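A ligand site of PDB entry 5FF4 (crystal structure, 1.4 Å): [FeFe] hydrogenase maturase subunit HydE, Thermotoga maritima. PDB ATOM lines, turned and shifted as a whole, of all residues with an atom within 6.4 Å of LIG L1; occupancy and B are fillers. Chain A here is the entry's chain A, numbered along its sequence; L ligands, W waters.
The side-chain hydroxyl (OH) of Tyr 316 is in hydrogen-bond range of the backbone NH (N) of Ala 280 (3.2 Å).
NE of Arg 169 is in hydrogen-bond range of O of Gly 236 (3.3 Å).
The side-chain hydroxyl of Thr 278 is in hydrogen-bond range of the backbone carbonyl oxygen of Ile 237, at 3.1 Å.
The side-chain hydroxyl of Thr 278 is in hydrogen-bond range of the backbone NH of Met 281, 3.5 Å away.
OE1 of Gln 117 sits at hydrogen-bond distance from OH of Tyr 313, 3.2 Å away.
The side-chain hydroxyl of Ser 146 lies within hydrogen-bond range of the side-chain amide nitrogen of Gln 117 (3.2 Å).
The side-chain hydroxyl (OG) of Ser 146 is in hydrogen-bond range of the backbone carbonyl oxygen (O) of Leu 167.
Water W2 lies within hydrogen-bond range of O3 of LIG L1 and NE of Arg 169.
Water W1 lies within hydrogen-bond range of an oxygen (O1) of LIG L1 (2.8 Å), the guanidinium group of Arg 169 (2.8 Å) and the side-chain hydroxyl of Thr 278 (3.1 Å).
Water W5 bridges a nitrogen (N1) of LIG L1 (2.8 Å) and the backbone NH (N) of Thr 279 (2.9 Å).
Water W3 bridges the side-chain carboxylate of Glu 68 and the side-chain amide oxygen of Gln 117.
O3 of LIG L1 sits close to SD of Met 301, 3.6 Å away.
CD1 of Ile 66 touches C5 of LIG L1 (3.6 Å).
Leu 167 touches LIG L1.
CA of Gly 236 touches O4 of LIG L1, 3.7 Å away.
Thr 278 touches LIG L1.
Leu 315 touches LIG L1 (CD1 to C7, 3.4 Å).
Hydrophobic or aromatic side chains that line LIG L1: Ile 66, Leu 167, Ala 280, Met 301, Leu 315 and Tyr 316.
Of the 21 residues printed, 11 come within 4 Å of LIG L1.
An oxygen (O2) of LIG L1 sits at hydrogen-bond distance from the side-chain hydroxyl (OH) of Tyr 316.
An oxygen (O4) of LIG L1 is in salt-bridge range of the guanidinium group of Arg 169 (2.7 Å).
An oxygen (O1) of LIG L1 sits at hydrogen-bond distance from the backbone NH of Ala 280, at 3.0 Å.
An oxygen (O1) of LIG L1 sits at hydrogen-bond distance from the backbone NH (N) of Thr 279, at 3.3 Å.
S1 of LIG L1 sits close to NE2 of Gln 117, 3.7 Å away.
The guanidinium group (NH1) of Arg 169 sits at hydrogen-bond distance from an oxygen (O5) of LG2 L2 (3.1 Å).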
ATOM      1  N   ILE A  66      10.253  20.717 -20.601  1.00  0.00           N
ATOM      2  CA  ILE A  66      10.411  20.492 -19.174  1.00  0.00           C
ATOM      3  C   ILE A  66      10.395  19.059 -18.772  1.00  0.00           C
ATOM      4  O   ILE A  66       9.489  18.338 -19.125  1.00  0.00           O
ATOM      5  CB  ILE A  66       9.306  21.206 -18.305  1.00  0.00           C
ATOM      6  CG1 ILE A  66       9.058  22.597 -18.645  1.00  0.00           C
ATOM      7  CG2 ILE A  66       9.582  21.082 -16.823  1.00  0.00           C
ATOM      8  CD1 ILE A  66       8.013  23.252 -17.813  1.00  0.00           C
ATOM      9  N   GLU A  68      10.254  17.041 -15.317  1.00  0.00           N
ATOM     10  CA  GLU A  68       9.924  17.164 -13.870  1.00  0.00           C
ATOM     11  C   GLU A  68      10.462  15.857 -13.291  1.00  0.00           C
ATOM     12  O   GLU A  68       9.798  14.824 -13.280  1.00  0.00           O
ATOM     13  CB  GLU A  68       8.446  17.351 -13.668  1.00  0.00           C
ATOM     14  CG  GLU A  68       7.853  18.528 -14.367  1.00  0.00           C
ATOM     15  CD  GLU A  68       6.377  18.369 -14.695  1.00  0.00           C
ATOM     16  OE1 GLU A  68       5.959  17.203 -15.011  1.00  0.00           O
ATOM     17  OE2 GLU A  68       5.627  19.326 -14.672  1.00  0.00           O
ATOM     18  N   VAL A 115      14.556  22.226 -19.660  1.00  0.00           N
ATOM     19  CA  VAL A 115      14.284  22.678 -18.310  1.00  0.00           C
ATOM     20  C   VAL A 115      14.249  21.472 -17.396  1.00  0.00           C
ATOM     21  O   VAL A 115      13.430  20.588 -17.613  1.00  0.00           O
ATOM     22  CB  VAL A 115      12.965  23.491 -18.191  1.00  0.00           C
ATOM     23  CG1 VAL A 115      12.762  23.966 -16.765  1.00  0.00           C
ATOM     24  CG2 VAL A 115      12.897  24.637 -19.170  1.00  0.00           C
ATOM     25  N   GLN A 117      13.167  20.541 -13.697  1.00  0.00           N
ATOM     26  CA  GLN A 117      12.381  21.042 -12.601  1.00  0.00           C
ATOM     27  C   GLN A 117      12.101  19.928 -11.598  1.00  0.00           C
ATOM     28  O   GLN A 117      11.866  18.803 -11.991  1.00  0.00           O
ATOM     29  CB  GLN A 117      11.068  21.704 -13.053  1.00  0.00           C
ATOM     30  CG  GLN A 117      10.348  22.478 -11.971  1.00  0.00           C
ATOM     31  CD  GLN A 117       9.131  23.181 -12.418  1.00  0.00           C
ATOM     32  OE1 GLN A 117       8.070  22.496 -12.562  1.00  0.00           O
ATOM     33  NE2 GLN A 117       9.143  24.417 -12.625  1.00  0.00           N
ATOM     34  N   SER A 146      15.233  24.607 -12.448  1.00  0.00           N
ATOM     35  CA  SER A 146      14.181  25.188 -11.593  1.00  0.00           C
ATOM     36  C   SER A 146      14.031  24.220 -10.422  1.00  0.00           C
ATOM     37  O   SER A 146      13.145  23.385 -10.361  1.00  0.00           O
ATOM     38  CB  SER A 146      12.895  25.240 -12.410  1.00  0.00           C
ATOM     39  OG  SER A 146      11.804  25.815 -11.666  1.00  0.00           O
ATOM     40  N   LEU A 167      15.031  29.357 -13.109  1.00  0.00           N
ATOM     41  CA  LEU A 167      13.709  29.849 -12.827  1.00  0.00           C
ATOM     42  C   LEU A 167      13.463  29.757 -11.349  1.00  0.00           C
ATOM     43  O   LEU A 167      13.524  28.662 -10.765  1.00  0.00           O
ATOM     44  CB  LEU A 167      12.646  29.028 -13.544  1.00  0.00           C
ATOM     45  CG  LEU A 167      12.903  28.851 -15.075  1.00  0.00           C
ATOM     46  CD1 LEU A 167      11.796  27.821 -15.548  1.00  0.00           C
ATOM     47  CD2 LEU A 167      12.990  30.209 -15.808  1.00  0.00           C
ATOM     48  N   ARG A 169      10.466  31.655  -9.308  1.00  0.00           N
ATOM     49  CA  ARG A 169       9.395  32.654  -9.171  1.00  0.00           C
ATOM     50  C   ARG A 169       9.459  33.266  -7.805  1.00  0.00           C
ATOM     51  O   ARG A 169       9.676  32.618  -6.801  1.00  0.00           O
ATOM     52  CB  ARG A 169       8.055  31.989  -9.308  1.00  0.00           C
ATOM     53  CG  ARG A 169       7.756  31.633 -10.766  1.00  0.00           C
ATOM     54  CD  ARG A 169       6.386  30.949 -10.679  1.00  0.00           C
ATOM     55  NE  ARG A 169       5.974  30.664 -12.011  1.00  0.00           N
ATOM     56  CZ  ARG A 169       4.669  30.491 -12.308  1.00  0.00           C
ATOM     57  NH1 ARG A 169       3.738  30.472 -11.298  1.00  0.00           N
ATOM     58  NH2 ARG A 169       4.343  30.340 -13.516  1.00  0.00           N
ATOM     59  N   VAL A 235       9.837  35.963 -16.992  1.00  0.00           N
ATOM     60  CA  VAL A 235       8.797  36.190 -15.983  1.00  0.00           C
ATOM     61  C   VAL A 235       7.687  35.163 -16.180  1.00  0.00           C
ATOM     62  O   VAL A 235       6.985  35.225 -17.226  1.00  0.00           O
ATOM     63  CB  VAL A 235       8.164  37.578 -15.990  1.00  0.00           C
ATOM     64  CG1 VAL A 235       7.161  37.741 -14.889  1.00  0.00           C
ATOM     65  CG2 VAL A 235       9.263  38.633 -15.870  1.00  0.00           C
ATOM     66  N   GLY A 236       7.527  34.218 -15.245  1.00  0.00           N
ATOM     67  CA  GLY A 236       6.501  33.217 -15.281  1.00  0.00           C
ATOM     68  C   GLY A 236       5.337  33.610 -14.346  1.00  0.00           C
ATOM     69  O   GLY A 236       5.516  33.735 -13.170  1.00  0.00           O
ATOM     70  N   ILE A 237       4.136  33.691 -14.989  1.00  0.00           N
ATOM     71  CA  ILE A 237       2.947  34.128 -14.228  1.00  0.00           C
ATOM     72  C   ILE A 237       1.802  33.174 -14.510  1.00  0.00           C
ATOM     73  O   ILE A 237       1.591  32.745 -15.692  1.00  0.00           O
ATOM     74  CB  ILE A 237       2.513  35.544 -14.687  1.00  0.00           C
ATOM     75  CG1 ILE A 237       3.550  36.555 -14.146  1.00  0.00           C
ATOM     76  CG2 ILE A 237       1.138  35.898 -14.139  1.00  0.00           C
ATOM     77  CD1 ILE A 237       3.440  37.901 -14.772  1.00  0.00           C
ATOM     78  N   GLY A 238       1.106  32.742 -13.521  1.00  0.00           N
ATOM     79  CA  GLY A 238      -0.057  31.989 -13.699  1.00  0.00           C
ATOM     80  C   GLY A 238      -0.999  32.190 -12.525  1.00  0.00           C
ATOM     81  O   GLY A 238      -0.632  32.737 -11.514  1.00  0.00           O
ATOM     82  N   PRO A 276       6.533  33.165 -20.607  1.00  0.00           N
ATOM     83  CA  PRO A 276       5.756  32.018 -21.062  1.00  0.00           C
ATOM     84  C   PRO A 276       4.293  32.150 -20.967  1.00  0.00           C
ATOM     85  O   PRO A 276       3.740  32.922 -20.131  1.00  0.00           O
ATOM     86  CB  PRO A 276       6.226  30.890 -20.145  1.00  0.00           C
ATOM     87  CG  PRO A 276       6.584  31.621 -18.874  1.00  0.00           C
ATOM     88  CD  PRO A 276       7.268  32.874 -19.362  1.00  0.00           C
ATOM     89  N   THR A 278       1.774  29.958 -19.664  1.00  0.00           N
ATOM     90  CA  THR A 278       2.013  28.841 -18.758  1.00  0.00           C
ATOM     91  C   THR A 278       0.978  27.768 -18.792  1.00  0.00           C
ATOM     92  O   THR A 278      -0.127  27.991 -19.176  1.00  0.00           O
ATOM     93  CB  THR A 278       2.124  29.322 -17.332  1.00  0.00           C
ATOM     94  OG1 THR A 278       0.924  29.983 -16.915  1.00  0.00           O
ATOM     95  CG2 THR A 278       3.314  30.271 -17.147  1.00  0.00           C
ATOM     96  N   THR A 279       1.406  26.567 -18.422  1.00  0.00           N
ATOM     97  CA  THR A 279       0.465  25.470 -18.351  1.00  0.00           C
ATOM     98  C   THR A 279      -0.658  25.794 -17.412  1.00  0.00           C
ATOM     99  O   THR A 279      -1.751  25.392 -17.707  1.00  0.00           O
ATOM    100  CB  THR A 279       1.189  24.146 -17.981  1.00  0.00           C
ATOM    101  OG1 THR A 279       2.012  23.766 -19.069  1.00  0.00           O
ATOM    102  CG2 THR A 279       0.224  23.022 -17.749  1.00  0.00           C
ATOM    103  N   ALA A 280      -0.449  26.495 -16.354  1.00  0.00           N
ATOM    104  CA  ALA A 280      -1.566  26.875 -15.449  1.00  0.00           C
ATOM    105  C   ALA A 280      -2.628  27.715 -16.150  1.00  0.00           C
ATOM    106  O   ALA A 280      -3.780  27.466 -15.922  1.00  0.00           O
ATOM    107  CB  ALA A 280      -1.013  27.568 -14.209  1.00  0.00           C
ATOM    108  N   MET A 281      -2.268  28.629 -17.052  1.00  0.00           N
ATOM    109  CA  MET A 281      -3.231  29.357 -17.869  1.00  0.00           C
ATOM    110  C   MET A 281      -4.086  28.430 -18.756  1.00  0.00           C
ATOM    111  O   MET A 281      -5.224  28.694 -18.935  1.00  0.00           O
ATOM    112  CB  MET A 281      -2.519  30.442 -18.701  1.00  0.00           C
ATOM    113  CG  MET A 281      -2.049  31.610 -17.860  1.00  0.00           C
ATOM    114  SD  MET A 281      -3.321  32.549 -17.090  1.00  0.00           S
ATOM    115  CE  MET A 281      -3.331  33.915 -18.259  1.00  0.00           C
ATOM    116  N   MET A 301       6.243  26.020 -22.759  1.00  0.00           N
ATOM    117  CA  MET A 301       7.005  25.045 -22.046  1.00  0.00           C
ATOM    118  C   MET A 301       6.310  23.642 -22.069  1.00  0.00           C
ATOM    119  O   MET A 301       5.762  23.285 -20.993  1.00  0.00           O
ATOM    120  CB  MET A 301       7.329  25.604 -20.612  1.00  0.00           C
ATOM    121  CG  MET A 301       7.894  27.080 -20.723  1.00  0.00           C
ATOM    122  SD  MET A 301       8.225  27.951 -19.197  1.00  0.00           S
ATOM    123  CE  MET A 301       9.609  26.978 -18.728  1.00  0.00           C
ATOM    124  N   TYR A 313       3.313  14.363 -10.874  1.00  0.00           N
ATOM    125  CA  TYR A 313       3.850  15.691 -10.617  1.00  0.00           C
ATOM    126  C   TYR A 313       2.725  16.708 -10.588  1.00  0.00           C
ATOM    127  O   TYR A 313       2.471  17.426 -11.524  1.00  0.00           O
ATOM    128  CB  TYR A 313       4.900  16.126 -11.595  1.00  0.00           C
ATOM    129  CG  TYR A 313       5.780  17.276 -11.135  1.00  0.00           C
ATOM    130  CD1 TYR A 313       6.886  17.115 -10.379  1.00  0.00           C
ATOM    131  CD2 TYR A 313       5.465  18.555 -11.488  1.00  0.00           C
ATOM    132  CE1 TYR A 313       7.722  18.142 -10.035  1.00  0.00           C
ATOM    133  CE2 TYR A 313       6.291  19.589 -11.151  1.00  0.00           C
ATOM    134  CZ  TYR A 313       7.347  19.365 -10.414  1.00  0.00           C
ATOM    135  OH  TYR A 313       8.154  20.407 -10.084  1.00  0.00           O
ATOM    136  N   LEU A 315       1.501  19.784  -8.914  1.00  0.00           N
ATOM    137  CA  LEU A 315       1.540  20.922  -8.114  1.00  0.00           C
ATOM    138  C   LEU A 315       0.109  21.458  -7.890  1.00  0.00           C
ATOM    139  O   LEU A 315      -0.148  21.902  -6.794  1.00  0.00           O
ATOM    140  CB  LEU A 315       2.367  22.004  -8.862  1.00  0.00           C
ATOM    141  CG  LEU A 315       3.747  21.614  -9.244  1.00  0.00           C
ATOM    142  CD1 LEU A 315       4.238  22.700 -10.223  1.00  0.00           C
ATOM    143  CD2 LEU A 315       4.633  21.576  -8.059  1.00  0.00           C
ATOM    144  N   TYR A 316      -0.765  21.277  -8.906  1.00  0.00           N
ATOM    145  CA  TYR A 316      -2.112  21.689  -8.866  1.00  0.00           C
ATOM    146  C   TYR A 316      -2.902  20.690  -9.678  1.00  0.00           C
ATOM    147  O   TYR A 316      -2.306  20.024 -10.540  1.00  0.00           O
ATOM    148  CB  TYR A 316      -2.228  23.103  -9.389  1.00  0.00           C
ATOM    149  CG  TYR A 316      -1.607  23.369 -10.735  1.00  0.00           C
ATOM    150  CD1 TYR A 316      -2.277  23.043 -11.898  1.00  0.00           C
ATOM    151  CD2 TYR A 316      -0.366  23.932 -10.843  1.00  0.00           C
ATOM    152  CE1 TYR A 316      -1.702  23.228 -13.142  1.00  0.00           C
ATOM    153  CE2 TYR A 316       0.212  24.136 -12.099  1.00  0.00           C
ATOM    154  CZ  TYR A 316      -0.483  23.826 -13.205  1.00  0.00           C
ATOM    155  OH  TYR A 316       0.071  24.010 -14.462  1.00  0.00           O
ATOM    156  N   LYS A 319      -3.806  19.512 -14.121  1.00  0.00           N
ATOM    157  CA  LYS A 319      -2.600  19.935 -14.842  1.00  0.00           C
ATOM    158  C   LYS A 319      -2.461  19.235 -16.164  1.00  0.00           C
ATOM    159  O   LYS A 319      -2.674  18.050 -16.226  1.00  0.00           O
ATOM    160  CB  LYS A 319      -1.365  19.690 -13.935  1.00  0.00           C
ATOM    161  CG  LYS A 319      -0.127  20.220 -14.682  1.00  0.00           C
ATOM    162  CD  LYS A 319       0.999  19.904 -13.764  1.00  0.00           C
ATOM    163  CE  LYS A 319       0.909  20.626 -12.509  1.00  0.00           C
ATOM    164  NZ  LYS A 319       2.105  20.386 -11.767  1.00  0.00           N
HETATM  165  C1  LIG L   1       6.442  27.285 -15.310  1.00  0.00           C
HETATM  166  C2  LIG L   1       4.477  26.000 -14.874  1.00  0.00           C
HETATM  167  C3  LIG L   1       4.952  26.092 -13.427  1.00  0.00           C
HETATM  168  S1  LIG L   1       6.564  26.917 -13.500  1.00  0.00           S
HETATM  169  O1  LIG L   1       2.257  26.777 -15.204  1.00  0.00           O
HETATM  170  C4  LIG L   1       2.980  25.807 -14.975  1.00  0.00           C
HETATM  171  O2  LIG L   1       2.571  24.639 -14.806  1.00  0.00           O
HETATM  172  N1  LIG L   1       5.038  27.134 -15.631  1.00  0.00           N
HETATM  173  C5  LIG L   1       7.270  26.256 -16.043  1.00  0.00           C
HETATM  174  C6  LIG L   1       6.866  28.700 -15.606  1.00  0.00           C
HETATM  175  O3  LIG L   1       8.088  28.907 -15.752  1.00  0.00           O
HETATM  176  O4  LIG L   1       6.033  29.573 -15.449  1.00  0.00           O
HETATM  177  C7  LIG L   1       5.124  24.748 -12.786  1.00  0.00           C
HETATM  178  C8  LIG L   1       3.957  26.956 -12.579  1.00  0.00           C
HETATM  179  N1  LG2 L   2      10.259  23.701  -6.171  1.00  0.00           N
HETATM  180  C1  LG2 L   2      10.693  24.700  -7.207  1.00  0.00           C
HETATM  181  C2  LG2 L   2      10.107  24.253  -8.539  1.00  0.00           C
HETATM  182  C3  LG2 L   2       8.744  23.551  -8.630  1.00  0.00           C
HETATM  183  S1  LG2 L   2       7.339  24.521  -8.116  1.00  0.00           S
HETATM  184  C4  LG2 L   2      10.167  25.992  -6.738  1.00  0.00           C
HETATM  185  O1  LG2 L   2      10.656  27.031  -7.308  1.00  0.00           O
HETATM  186  O2  LG2 L   2       9.323  26.114  -5.767  1.00  0.00           O
HETATM  187  C5  LG2 L   2       7.238  25.676  -9.493  1.00  0.00           C
HETATM  188  C6  LG2 L   2       6.114  26.732  -9.357  1.00  0.00           C
HETATM  189  O3  LG2 L   2       4.803  26.103  -9.257  1.00  0.00           O
HETATM  190  C7  LG2 L   2       6.105  27.620  -8.137  1.00  0.00           C
HETATM  191  O4  LG2 L   2       7.072  28.649  -8.298  1.00  0.00           O
HETATM  192  C8  LG2 L   2       4.635  28.125  -8.004  1.00  0.00           C
HETATM  193  O5  LG2 L   2       4.427  29.440  -8.498  1.00  0.00           O
HETATM  194  C9  LG2 L   2       3.838  27.106  -8.877  1.00  0.00           C
HETATM  195  N2  LG2 L   2       2.798  26.428  -8.197  1.00  0.00           N
HETATM  196  C10 LG2 L   2       2.949  25.629  -7.125  1.00  0.00           C
HETATM  197  N3  LG2 L   2       1.716  25.260  -6.631  1.00  0.00           N
HETATM  198  C11 LG2 L   2       0.756  25.916  -7.411  1.00  0.00           C
HETATM  199  C12 LG2 L   2      -0.638  25.922  -7.418  1.00  0.00           C
HETATM  200  N4  LG2 L   2      -1.362  25.305  -6.489  1.00  0.00           N
HETATM  201  N5  LG2 L   2      -1.258  26.700  -8.349  1.00  0.00           N
HETATM  202  C13 LG2 L   2      -0.563  27.288  -9.356  1.00  0.00           C
HETATM  203  N6  LG2 L   2       0.802  27.308  -9.381  1.00  0.00           N
HETATM  204  C14 LG2 L   2       1.471  26.607  -8.471  1.00  0.00           C
HETATM  205  O   HOH W   1       1.804  29.256 -13.987  1.00  0.00           O
HETATM  206  O   HOH W   2       8.859  29.965 -13.383  1.00  0.00           O
HETATM  207  O   HOH W   3       6.199  21.897 -14.415  1.00  0.00           O
HETATM  208  O   HOH W   4       4.361  22.665 -15.917  1.00  0.00           O
HETATM  209  O   HOH W   5       4.285  26.326 -18.244  1.00  0.00           O
HETATM  210  O   HOH W   6       9.292  31.353 -16.628  1.00  0.00           O
